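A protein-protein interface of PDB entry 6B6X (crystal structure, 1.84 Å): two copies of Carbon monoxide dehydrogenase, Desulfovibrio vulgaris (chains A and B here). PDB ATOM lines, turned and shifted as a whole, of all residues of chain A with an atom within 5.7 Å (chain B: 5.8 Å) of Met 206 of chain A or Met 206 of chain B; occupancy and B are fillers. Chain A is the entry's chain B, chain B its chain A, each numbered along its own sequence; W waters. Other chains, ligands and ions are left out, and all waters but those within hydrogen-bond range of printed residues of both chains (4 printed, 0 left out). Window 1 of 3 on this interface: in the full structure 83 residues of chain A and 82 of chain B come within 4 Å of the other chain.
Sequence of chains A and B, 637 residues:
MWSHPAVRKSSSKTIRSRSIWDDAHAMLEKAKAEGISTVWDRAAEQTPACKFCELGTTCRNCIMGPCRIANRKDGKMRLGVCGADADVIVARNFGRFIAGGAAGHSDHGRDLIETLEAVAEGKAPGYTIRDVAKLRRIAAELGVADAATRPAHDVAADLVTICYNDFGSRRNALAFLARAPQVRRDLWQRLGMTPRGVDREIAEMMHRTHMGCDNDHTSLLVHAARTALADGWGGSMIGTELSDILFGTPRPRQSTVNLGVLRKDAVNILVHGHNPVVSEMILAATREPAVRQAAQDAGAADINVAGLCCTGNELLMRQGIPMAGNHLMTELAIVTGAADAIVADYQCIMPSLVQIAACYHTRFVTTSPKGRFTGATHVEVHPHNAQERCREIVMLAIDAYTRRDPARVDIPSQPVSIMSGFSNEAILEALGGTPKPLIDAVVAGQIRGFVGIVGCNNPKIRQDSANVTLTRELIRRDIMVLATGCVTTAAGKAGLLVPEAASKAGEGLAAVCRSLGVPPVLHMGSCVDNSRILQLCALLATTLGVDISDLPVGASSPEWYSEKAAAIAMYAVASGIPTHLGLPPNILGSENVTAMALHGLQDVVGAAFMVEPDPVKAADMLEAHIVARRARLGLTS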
ATOM      1  N   ARG A  96       2.021   2.188 -12.511  1.00  0.00           N
ATOM      2  CA  ARG A  96       2.552   0.891 -12.086  1.00  0.00           C
ATOM      3  C   ARG A  96       3.872   1.055 -11.343  1.00  0.00           C
ATOM      4  O   ARG A  96       4.156   0.307 -10.401  1.00  0.00           O
ATOM      5  CB  ARG A  96       2.720  -0.049 -13.283  1.00  0.00           C
ATOM      6  CG  ARG A  96       1.389  -0.522 -13.869  1.00  0.00           C
ATOM      7  CD  ARG A  96       1.512  -1.804 -14.696  1.00  0.00           C
ATOM      8  NE  ARG A  96       0.187  -2.376 -14.954  1.00  0.00           N
ATOM      9  CZ  ARG A  96      -0.035  -3.495 -15.637  1.00  0.00           C
ATOM     10  NH1 ARG A  96      -1.279  -3.931 -15.804  1.00  0.00           N
ATOM     11  NH2 ARG A  96       0.982  -4.181 -16.150  1.00  0.00           N
ATOM     12  N   ALA A  99       2.933   1.965  -7.900  1.00  0.00           N
ATOM     13  CA  ALA A  99       2.339   0.825  -7.207  1.00  0.00           C
ATOM     14  C   ALA A  99       3.403  -0.154  -6.734  1.00  0.00           C
ATOM     15  O   ALA A  99       3.265  -0.765  -5.668  1.00  0.00           O
ATOM     16  CB  ALA A  99       1.331   0.117  -8.110  1.00  0.00           C
ATOM     17  N   GLY A 100       4.471  -0.323  -7.516  1.00  0.00           N
ATOM     18  CA  GLY A 100       5.563  -1.178  -7.073  1.00  0.00           C
ATOM     19  C   GLY A 100       6.255  -0.643  -5.834  1.00  0.00           C
ATOM     20  O   GLY A 100       6.646  -1.409  -4.946  1.00  0.00           O
ATOM     21  N   ALA A 103       3.928  -1.152  -2.918  1.00  0.00           N
ATOM     22  CA  ALA A 103       3.863  -2.569  -2.569  1.00  0.00           C
ATOM     23  C   ALA A 103       5.056  -2.998  -1.724  1.00  0.00           C
ATOM     24  O   ALA A 103       4.923  -3.860  -0.847  1.00  0.00           O
ATOM     25  CB  ALA A 103       3.790  -3.423  -3.836  1.00  0.00           C
ATOM     26  N   GLY A 104       6.229  -2.430  -1.990  1.00  0.00           N
ATOM     27  CA  GLY A 104       7.385  -2.740  -1.165  1.00  0.00           C
ATOM     28  C   GLY A 104       7.168  -2.362   0.287  1.00  0.00           C
ATOM     29  O   GLY A 104       7.380  -3.171   1.192  1.00  0.00           O
ATOM     30  N   GLU A 201      -5.552  -0.485  -3.045  1.00  0.00           N
ATOM     31  CA  GLU A 201      -5.163   0.554  -3.998  1.00  0.00           C
ATOM     32  C   GLU A 201      -4.133   0.030  -4.988  1.00  0.00           C
ATOM     33  O   GLU A 201      -4.147   0.410  -6.164  1.00  0.00           O
ATOM     34  CB  GLU A 201      -4.621   1.797  -3.279  1.00  0.00           C
ATOM     35  CG  GLU A 201      -5.489   2.361  -2.140  1.00  0.00           C
ATOM     36  CD  GLU A 201      -6.955   2.582  -2.503  1.00  0.00           C
ATOM     37  OE1 GLU A 201      -7.773   2.661  -1.564  1.00  0.00           O
ATOM     38  OE2 GLU A 201      -7.300   2.677  -3.700  1.00  0.00           O
ATOM     39  N   ILE A 202      -3.234  -0.844  -4.530  1.00  0.00           N
ATOM     40  CA  ILE A 202      -2.248  -1.442  -5.426  1.00  0.00           C
ATOM     41  C   ILE A 202      -2.944  -2.315  -6.462  1.00  0.00           C
ATOM     42  O   ILE A 202      -2.665  -2.230  -7.664  1.00  0.00           O
ATOM     43  CB  ILE A 202      -1.206  -2.243  -4.622  1.00  0.00           C
ATOM     44  CG1 ILE A 202      -0.383  -1.309  -3.734  1.00  0.00           C
ATOM     45  CG2 ILE A 202      -0.302  -3.041  -5.558  1.00  0.00           C
ATOM     46  CD1 ILE A 202       0.286  -2.008  -2.557  1.00  0.00           C
ATOM     47  N   ALA A 203      -3.868  -3.163  -6.011  1.00  0.00           N
ATOM     48  CA  ALA A 203      -4.591  -4.019  -6.945  1.00  0.00           C
ATOM     49  C   ALA A 203      -5.399  -3.189  -7.938  1.00  0.00           C
ATOM     50  O   ALA A 203      -5.425  -3.497  -9.135  1.00  0.00           O
ATOM     51  CB  ALA A 203      -5.499  -4.983  -6.182  1.00  0.00           C
ATOM     52  N   GLU A 204      -6.052  -2.122  -7.464  1.00  0.00           N
ATOM     53  CA  GLU A 204      -6.827  -1.285  -8.376  1.00  0.00           C
ATOM     54  C   GLU A 204      -5.925  -0.591  -9.385  1.00  0.00           C
ATOM     55  O   GLU A 204      -6.308  -0.422 -10.548  1.00  0.00           O
ATOM     56  CB  GLU A 204      -7.655  -0.250  -7.610  1.00  0.00           C
ATOM     57  CG  GLU A 204      -8.484   0.631  -8.561  1.00  0.00           C
ATOM     58  CD  GLU A 204      -9.454   1.561  -7.857  1.00  0.00           C
ATOM     59  OE1 GLU A 204     -10.205   1.098  -6.969  1.00  0.00           O
ATOM     60  OE2 GLU A 204      -9.468   2.758  -8.206  1.00  0.00           O
ATOM     61  N   MET A 205      -4.714  -0.196  -8.973  1.00  0.00           N
ATOM     62  CA  MET A 205      -3.800   0.414  -9.933  1.00  0.00           C
ATOM     63  C   MET A 205      -3.449  -0.565 -11.046  1.00  0.00           C
ATOM     64  O   MET A 205      -3.418  -0.192 -12.224  1.00  0.00           O
ATOM     65  CB  MET A 205      -2.528   0.913  -9.244  1.00  0.00           C
ATOM     66  CG  MET A 205      -1.533   1.528 -10.227  1.00  0.00           C
ATOM     67  SD  MET A 205      -2.192   2.952 -11.137  1.00  0.00           S
ATOM     68  CE  MET A 205      -1.815   4.228  -9.966  1.00  0.00           C
ATOM     69  N   MET A 206      -3.186  -1.827 -10.691  1.00  0.00           N
ATOM     70  CA  MET A 206      -2.872  -2.824 -11.706  1.00  0.00           C
ATOM     71  C   MET A 206      -4.072  -3.110 -12.599  1.00  0.00           C
ATOM     72  O   MET A 206      -3.901  -3.397 -13.789  1.00  0.00           O
ATOM     73  CB  MET A 206      -2.366  -4.108 -11.042  1.00  0.00           C
ATOM     74  CG  MET A 206      -1.081  -3.902 -10.251  1.00  0.00           C
ATOM     75  SD  MET A 206       0.255  -3.274 -11.284  1.00  0.00           S
ATOM     76  CE  MET A 206       0.573  -4.696 -12.331  1.00  0.00           C
ATOM     77  N   HIS A 207      -5.287  -3.032 -12.054  1.00  0.00           N
ATOM     78  CA  HIS A 207      -6.477  -3.144 -12.891  1.00  0.00           C
ATOM     79  C   HIS A 207      -6.607  -1.944 -13.825  1.00  0.00           C
ATOM     80  O   HIS A 207      -6.824  -2.104 -15.034  1.00  0.00           O
ATOM     81  CB  HIS A 207      -7.715  -3.282 -12.008  1.00  0.00           C
ATOM     82  CG  HIS A 207      -9.011  -3.225 -12.757  1.00  0.00           C
ATOM     83  ND1 HIS A 207     -10.171  -2.752 -12.187  1.00  0.00           N
ATOM     84  CD2 HIS A 207      -9.332  -3.586 -14.023  1.00  0.00           C
ATOM     85  CE1 HIS A 207     -11.156  -2.825 -13.067  1.00  0.00           C
ATOM     86  NE2 HIS A 207     -10.671  -3.323 -14.191  1.00  0.00           N
ATOM     87  N   ARG A 208      -6.467  -0.728 -13.281  1.00  0.00           N
ATOM     88  CA  ARG A 208      -6.653   0.475 -14.087  1.00  0.00           C
ATOM     89  C   ARG A 208      -5.698   0.516 -15.266  1.00  0.00           C
ATOM     90  O   ARG A 208      -6.038   1.065 -16.322  1.00  0.00           O
ATOM     91  CB  ARG A 208      -6.463   1.727 -13.228  1.00  0.00           C
ATOM     92  CG  ARG A 208      -7.638   2.063 -12.329  1.00  0.00           C
ATOM     93  CD  ARG A 208      -7.358   3.320 -11.510  1.00  0.00           C
ATOM     94  NE  ARG A 208      -8.473   3.613 -10.615  1.00  0.00           N
ATOM     95  CZ  ARG A 208      -9.429   4.494 -10.880  1.00  0.00           C
ATOM     96  NH1 ARG A 208     -10.413   4.686 -10.011  1.00  0.00           N
ATOM     97  NH2 ARG A 208      -9.401   5.180 -12.016  1.00  0.00           N
ATOM     98  N   THR A 209      -4.508  -0.058 -15.111  1.00  0.00           N
ATOM     99  CA  THR A 209      -3.476   0.005 -16.134  1.00  0.00           C
ATOM    100  C   THR A 209      -3.528  -1.163 -17.117  1.00  0.00           C
ATOM    101  O   THR A 209      -2.726  -1.191 -18.054  1.00  0.00           O
ATOM    102  CB  THR A 209      -2.098   0.079 -15.473  1.00  0.00           C
ATOM    103  OG1 THR A 209      -1.960  -0.997 -14.541  1.00  0.00           O
ATOM    104  CG2 THR A 209      -1.945   1.403 -14.735  1.00  0.00           C
ATOM    105  N   HIS A 210      -4.441  -2.116 -16.922  1.00  0.00           N
ATOM    106  CA  HIS A 210      -4.742  -3.114 -17.945  1.00  0.00           C
ATOM    107  C   HIS A 210      -5.280  -2.420 -19.193  1.00  0.00           C
ATOM    108  O   HIS A 210      -5.867  -1.336 -19.115  1.00  0.00           O
ATOM    109  CB  HIS A 210      -5.773  -4.117 -17.405  1.00  0.00           C
ATOM    110  CG  HIS A 210      -5.978  -5.329 -18.267  1.00  0.00           C
ATOM    111  ND1 HIS A 210      -6.656  -5.291 -19.467  1.00  0.00           N
ATOM    112  CD2 HIS A 210      -5.615  -6.622 -18.084  1.00  0.00           C
ATOM    113  CE1 HIS A 210      -6.688  -6.503 -19.994  1.00  0.00           C
ATOM    114  NE2 HIS A 210      -6.062  -7.330 -19.174  1.00  0.00           N
ATOM    115  N   GLU A 563      11.453   2.608  -7.102  1.00  0.00           N
ATOM    116  CA  GLU A 563      10.010   2.828  -7.112  1.00  0.00           C
ATOM    117  C   GLU A 563       9.513   3.275  -5.742  1.00  0.00           C
ATOM    118  O   GLU A 563       8.592   4.096  -5.644  1.00  0.00           O
ATOM    119  CB  GLU A 563       9.289   1.553  -7.564  1.00  0.00           C
ATOM    120  CG  GLU A 563       9.443   1.269  -9.051  1.00  0.00           C
ATOM    121  CD  GLU A 563       8.871  -0.077  -9.474  1.00  0.00           C
ATOM    122  OE1 GLU A 563       8.927  -1.037  -8.680  1.00  0.00           O
ATOM    123  OE2 GLU A 563       8.377  -0.178 -10.615  1.00  0.00           O
ATOM    124  N   ARG B  96       4.615  -9.441 -13.350  1.00  0.00           N
ATOM    125  CA  ARG B  96       3.782  -8.240 -13.345  1.00  0.00           C
ATOM    126  C   ARG B  96       2.689  -8.325 -14.402  1.00  0.00           C
ATOM    127  O   ARG B  96       1.576  -7.826 -14.192  1.00  0.00           O
ATOM    128  CB  ARG B  96       4.640  -6.989 -13.557  1.00  0.00           C
ATOM    129  CG  ARG B  96       5.440  -6.582 -12.318  1.00  0.00           C
ATOM    130  CD  ARG B  96       5.926  -5.126 -12.345  1.00  0.00           C
ATOM    131  NE  ARG B  96       6.503  -4.768 -11.047  1.00  0.00           N
ATOM    132  CZ  ARG B  96       7.012  -3.581 -10.730  1.00  0.00           C
ATOM    133  NH1 ARG B  96       7.501  -3.380  -9.508  1.00  0.00           N
ATOM    134  NH2 ARG B  96       7.044  -2.601 -11.622  1.00  0.00           N
ATOM    135  N   ALA B  99       0.088 -10.402 -12.884  1.00  0.00           N
ATOM    136  CA  ALA B  99      -0.545  -9.657 -11.800  1.00  0.00           C
ATOM    137  C   ALA B  99      -1.583  -8.678 -12.337  1.00  0.00           C
ATOM    138  O   ALA B  99      -2.650  -8.504 -11.736  1.00  0.00           O
ATOM    139  CB  ALA B  99       0.510  -8.914 -10.978  1.00  0.00           C
ATOM    140  N   GLY B 100      -1.282  -8.019 -13.461  1.00  0.00           N
ATOM    141  CA  GLY B 100      -2.265  -7.130 -14.063  1.00  0.00           C
ATOM    142  C   GLY B 100      -3.518  -7.862 -14.500  1.00  0.00           C
ATOM    143  O   GLY B 100      -4.631  -7.339 -14.378  1.00  0.00           O
ATOM    144  N   ALA B 103      -5.489  -8.746 -11.379  1.00  0.00           N
ATOM    145  CA  ALA B 103      -6.078  -7.551 -10.786  1.00  0.00           C
ATOM    146  C   ALA B 103      -7.379  -7.160 -11.478  1.00  0.00           C
ATOM    147  O   ALA B 103      -8.314  -6.677 -10.829  1.00  0.00           O
ATOM    148  CB  ALA B 103      -5.083  -6.395 -10.850  1.00  0.00           C
ATOM    149  N   GLY B 104      -7.448  -7.334 -12.798  1.00  0.00           N
ATOM    150  CA  GLY B 104      -8.697  -7.066 -13.492  1.00  0.00           C
ATOM    151  C   GLY B 104      -9.831  -7.937 -12.984  1.00  0.00           C
ATOM    152  O   GLY B 104     -10.936  -7.455 -12.718  1.00  0.00           O
ATOM    153  N   GLU B 201      -1.862 -11.412  -2.994  1.00  0.00           N
ATOM    154  CA  GLU B 201      -0.908 -12.009  -3.925  1.00  0.00           C
ATOM    155  C   GLU B 201      -0.481 -11.011  -4.992  1.00  0.00           C
ATOM    156  O   GLU B 201       0.678 -11.008  -5.419  1.00  0.00           O
ATOM    157  CB  GLU B 201      -1.485 -13.271  -4.576  1.00  0.00           C
ATOM    158  CG  GLU B 201      -2.067 -14.324  -3.612  1.00  0.00           C
ATOM    159  CD  GLU B 201      -1.133 -14.756  -2.492  1.00  0.00           C
ATOM    160  OE1 GLU B 201      -1.641 -15.382  -1.542  1.00  0.00           O
ATOM    161  OE2 GLU B 201       0.090 -14.488  -2.549  1.00  0.00           O
ATOM    162  N   ILE B 202      -1.403 -10.148  -5.430  1.00  0.00           N
ATOM    163  CA  ILE B 202      -1.050  -9.123  -6.410  1.00  0.00           C
ATOM    164  C   ILE B 202      -0.048  -8.144  -5.813  1.00  0.00           C
ATOM    165  O   ILE B 202       0.988  -7.841  -6.417  1.00  0.00           O
ATOM    166  CB  ILE B 202      -2.315  -8.397  -6.904  1.00  0.00           C
ATOM    167  CG1 ILE B 202      -3.215  -9.364  -7.682  1.00  0.00           C
ATOM    168  CG2 ILE B 202      -1.929  -7.180  -7.754  1.00  0.00           C
ATOM    169  CD1 ILE B 202      -4.658  -8.902  -7.776  1.00  0.00           C
ATOM    170  N   ALA B 203      -0.345  -7.636  -4.614  1.00  0.00           N
ATOM    171  CA  ALA B 203       0.579  -6.717  -3.954  1.00  0.00           C
ATOM    172  C   ALA B 203       1.934  -7.374  -3.724  1.00  0.00           C
ATOM    173  O   ALA B 203       2.978  -6.747  -3.943  1.00  0.00           O
ATOM    174  CB  ALA B 203      -0.012  -6.234  -2.626  1.00  0.00           C
ATOM    175  N   GLU B 204       1.943  -8.637  -3.290  1.00  0.00           N
ATOM    176  CA  GLU B 204       3.226  -9.296  -3.081  1.00  0.00           C
ATOM    177  C   GLU B 204       3.984  -9.459  -4.391  1.00  0.00           C
ATOM    178  O   GLU B 204       5.217  -9.366  -4.407  1.00  0.00           O
ATOM    179  CB  GLU B 204       3.050 -10.655  -2.399  1.00  0.00           C
ATOM    180  CG  GLU B 204       4.405 -11.264  -2.006  1.00  0.00           C
ATOM    181  CD  GLU B 204       4.305 -12.635  -1.369  1.00  0.00           C
ATOM    182  OE1 GLU B 204       4.921 -13.581  -1.905  1.00  0.00           O
ATOM    183  OE2 GLU B 204       3.627 -12.762  -0.330  1.00  0.00           O
ATOM    184  N   MET B 205       3.278  -9.695  -5.501  1.00  0.00           N
ATOM    185  CA  MET B 205       3.976  -9.756  -6.781  1.00  0.00           C
ATOM    186  C   MET B 205       4.653  -8.431  -7.097  1.00  0.00           C
ATOM    187  O   MET B 205       5.787  -8.409  -7.585  1.00  0.00           O
ATOM    188  CB  MET B 205       3.028 -10.137  -7.918  1.00  0.00           C
ATOM    189  CG  MET B 205       3.755 -10.164  -9.280  1.00  0.00           C
ATOM    190  SD  MET B 205       5.081 -11.409  -9.369  1.00  0.00           S
ATOM    191  CE  MET B 205       4.093 -12.825  -9.748  1.00  0.00           C
ATOM    192  N   MET B 206       3.972  -7.313  -6.827  1.00  0.00           N
ATOM    193  CA  MET B 206       4.574  -6.017  -7.116  1.00  0.00           C
ATOM    194  C   MET B 206       5.762  -5.739  -6.205  1.00  0.00           C
ATOM    195  O   MET B 206       6.708  -5.062  -6.617  1.00  0.00           O
ATOM    196  CB  MET B 206       3.526  -4.914  -6.998  1.00  0.00           C
ATOM    197  CG  MET B 206       2.387  -5.077  -7.991  1.00  0.00           C
ATOM    198  SD  MET B 206       2.991  -5.048  -9.691  1.00  0.00           S
ATOM    199  CE  MET B 206       3.564  -3.361  -9.843  1.00  0.00           C
ATOM    200  N   HIS B 207       5.732  -6.254  -4.975  1.00  0.00           N
ATOM    201  CA  HIS B 207       6.893  -6.155  -4.097  1.00  0.00           C
ATOM    202  C   HIS B 207       8.040  -7.013  -4.611  1.00  0.00           C
ATOM    203  O   HIS B 207       9.181  -6.543  -4.719  1.00  0.00           O
ATOM    204  CB  HIS B 207       6.504  -6.573  -2.675  1.00  0.00           C
ATOM    205  CG  HIS B 207       7.664  -6.667  -1.729  1.00  0.00           C
ATOM    206  ND1 HIS B 207       7.650  -7.482  -0.619  1.00  0.00           N
ATOM    207  CD2 HIS B 207       8.867  -6.042  -1.720  1.00  0.00           C
ATOM    208  CE1 HIS B 207       8.789  -7.355   0.038  1.00  0.00           C
ATOM    209  NE2 HIS B 207       9.549  -6.494  -0.614  1.00  0.00           N
ATOM    210  N   ARG B 208       7.754  -8.278  -4.944  1.00  0.00           N
ATOM    211  CA  ARG B 208       8.809  -9.185  -5.393  1.00  0.00           C
ATOM    212  C   ARG B 208       9.526  -8.663  -6.628  1.00  0.00           C
ATOM    213  O   ARG B 208      10.714  -8.945  -6.817  1.00  0.00           O
ATOM    214  CB  ARG B 208       8.235 -10.571  -5.690  1.00  0.00           C
ATOM    215  CG  ARG B 208       7.905 -11.400  -4.461  1.00  0.00           C
ATOM    216  CD  ARG B 208       7.316 -12.761  -4.871  1.00  0.00           C
ATOM    217  NE  ARG B 208       6.957 -13.549  -3.695  1.00  0.00           N
ATOM    218  CZ  ARG B 208       7.730 -14.484  -3.157  1.00  0.00           C
ATOM    219  NH1 ARG B 208       8.909 -14.765  -3.701  1.00  0.00           N
ATOM    220  NH2 ARG B 208       7.323 -15.140  -2.077  1.00  0.00           N
ATOM    221  N   THR B 209       8.833  -7.909  -7.479  1.00  0.00           N
ATOM    222  CA  THR B 209       9.420  -7.451  -8.730  1.00  0.00           C
ATOM    223  C   THR B 209      10.080  -6.077  -8.620  1.00  0.00           C
ATOM    224  O   THR B 209      10.636  -5.597  -9.614  1.00  0.00           O
ATOM    225  CB  THR B 209       8.355  -7.457  -9.839  1.00  0.00           C
ATOM    226  OG1 THR B 209       7.194  -6.741  -9.405  1.00  0.00           O
ATOM    227  CG2 THR B 209       7.941  -8.889 -10.162  1.00  0.00           C
ATOM    228  N   HIS B 210      10.025  -5.438  -7.448  1.00  0.00           N
ATOM    229  CA  HIS B 210      10.855  -4.270  -7.164  1.00  0.00           C
ATOM    230  C   HIS B 210      12.328  -4.665  -7.226  1.00  0.00           C
ATOM    231  O   HIS B 210      12.688  -5.811  -6.939  1.00  0.00           O
ATOM    232  CB  HIS B 210      10.505  -3.710  -5.772  1.00  0.00           C
ATOM    233  CG  HIS B 210      11.133  -2.385  -5.451  1.00  0.00           C
ATOM    234  ND1 HIS B 210      12.470  -2.242  -5.147  1.00  0.00           N
ATOM    235  CD2 HIS B 210      10.592  -1.145  -5.351  1.00  0.00           C
ATOM    236  CE1 HIS B 210      12.731  -0.971  -4.896  1.00  0.00           C
ATOM    237  NE2 HIS B 210      11.608  -0.284  -5.012  1.00  0.00           N
ATOM    238  N   GLU B 563      -3.504  -9.425 -20.589  1.00  0.00           N
ATOM    239  CA  GLU B 563      -2.955  -9.925 -19.334  1.00  0.00           C
ATOM    240  C   GLU B 563      -3.941 -10.855 -18.639  1.00  0.00           C
ATOM    241  O   GLU B 563      -3.541 -11.840 -18.009  1.00  0.00           O
ATOM    242  CB  GLU B 563      -2.579  -8.751 -18.426  1.00  0.00           C
ATOM    243  CG  GLU B 563      -1.321  -8.023 -18.884  1.00  0.00           C
ATOM    244  CD  GLU B 563      -1.005  -6.784 -18.057  1.00  0.00           C
ATOM    245  OE1 GLU B 563      -1.942  -6.181 -17.496  1.00  0.00           O
ATOM    246  OE2 GLU B 563       0.187  -6.408 -17.976  1.00  0.00           O
HETATM  247  O   HOH W   1       7.933   0.061 -13.376  1.00  0.00           O
HETATM  248  O   HOH W   2      12.030  -1.255  -8.368  1.00  0.00           O
HETATM  249  O   HOH W   3      -3.615  -5.799 -20.372  1.00  0.00           O
HETATM  250  O   HOH W   4       2.828  -5.859 -18.326  1.00  0.00           O
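Water W4 lies within hydrogen-bond range of the side-chain carboxylate of Glu 563 of chain B (2.7 Å) and the guanidinium group of Arg 96 of chain A (3.3 Å). Water W1 lies within hydrogen-bond range of OE2 of Glu 563 of chain A (2.8 Å) and NH2 of Arg 96 of chain B (3.3 Å). Water W3 lies within hydrogen-bond range of a ring nitrogen (NE2) of His 210 of chain A (3.1 Å) and the side-chain carboxylate of Glu 563 of chain B (3.3 Å). Water W2 bridges OE1 of Glu 563 of chain A and ND1 of His 210 of chain B.
SD of Met 206 of chain A sits close to SD of Met 206 of chain B (3.6 Å). The guanidinium group (NH1) of Arg 96 of chain B lies within salt-bridge range of the side-chain carboxylate (OE1) of Glu 563 of chain A, at 2.9 Å. The side-chain carboxylate (OE1) of Glu 563 of chain B lies within salt-bridge range of the guanidinium group (NH1) of Arg 96 of chain A (2.9 Å).
Met 205 of chain A touches none of the printed residues of chain B. Met 206 of chain A touches just these residues of chain B: Arg 96 (3.8 Å), Gly 100 (3.97 Å), Ala 103 (3.6 Å) and Met 206 (3.6 Å). Of the printed residues of chain B, His 207 of chain A touches Ala 103 (3.6 Å) and Gly 104 (3.6 Å). Of the printed residues of chain A, Arg 96 of chain B touches Gly 100, Met 206 and Glu 563. Printed residues of chain A within 4 Å of Gly 100 of chain B: Arg 96 (3.8 Å), Met 206 (3.97 Å) and His 210 (3.9 Å). Met 206 of chain B touches four residues of chain A. Thr 209 of chain B touches none of the printed residues of chain A. The nearest residue of chain A that does not touch Met 206 of chain B is Ile 202 of chain A (4.2 Å). The nearest printed residue of chain A that does not touch Arg 96 of chain B is Arg 96 of chain A (4.2 Å).
The guanidinium group of Arg 96 of chain A is in hydrogen-bond range of the backbone carbonyl oxygen of Met 206 of chain A (3.3 Å). NE of Arg 96 of chain A lies within hydrogen-bond range of OG1 of Thr 209 of chain A (2.6 Å). O of Met 206 of chain B sits at hydrogen-bond distance from OG1 of Thr 209 of chain B (3.3 Å). The guanidinium group (NH1) of Arg 96 of chain B lies within hydrogen-bond range of the backbone carbonyl oxygen (O) of Met 206 of chain B (3.4 Å). OG1 of Thr 209 of chain B lies within hydrogen-bond range of NE of Arg 96 of chain B (2.7 Å). The side-chain hydroxyl (OG1) of Thr 209 of chain A lies within hydrogen-bond range of the backbone carbonyl oxygen (O) of Met 206 of chain A, 3.2 Å away.
Printed residues of chain A that touch a printed residue of chain B: Arg 96, Gly 100, Ala 103, Gly 104, Ala 203, Met 206, His 207, His 210 and Glu 563. Hydrophobic or aromatic side chains of chain A within 4 Å of the printed part of chain B: Ala 103, Met 206, His 207 and His 210. Among the printed residues, 21 pairs touch across the chains.
Arg 96 of chain A touches Met 206 of chain B. CE of Met 206 of chain B touches N of Gly 100 of chain A, at 3.9 Å. His 210 of chain B touches Gly 100 of chain A. Ala 103 of chain A touches His 207 of chain B (CB to N, 3.6 Å). O of Ala 203 of chain A touches CB of Ala 103 of chain B, at 3.4 Å. N of Gly 100 of chain B touches CE of Met 206 of chain A, 3.97 Å away. Ala 103 of chain B touches His 207 of chain A. CA of Gly 104 of chain B touches CD2 of His 207 of chain A (3.6 Å). CD2 of His 210 of chain A touches O of Gly 100 of chain B, 3.9 Å away. N of Glu 563 of chain A touches NE2 of His 210 of chain B, 3.6 Å away.
Gly 100 of chain A touches Met 206 of chain B, and with the chains exchanged Met 206 of chain A touches Gly 100 of chain B. Gly 100 of chain A touches His 210 of chain B, and with the chains exchanged His 210 of chain A touches Gly 100 of chain B. Ala 103 of chain A touches Met 206 of chain B, and with the chains exchanged Met 206 of chain A touches Ala 103 of chain B. Met 206 of chain B touches its own counterpart, Met 206 of chain A. Positions printed for both chains: 96, 99, 100, 103, 104, 201, 202, 203, 204, 205, 206, 207, 208, 209, 210 and 563. Of the 21 pairs that touch across the chains among the printed residues, 21 have their exchanged pair printed and touching as well.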
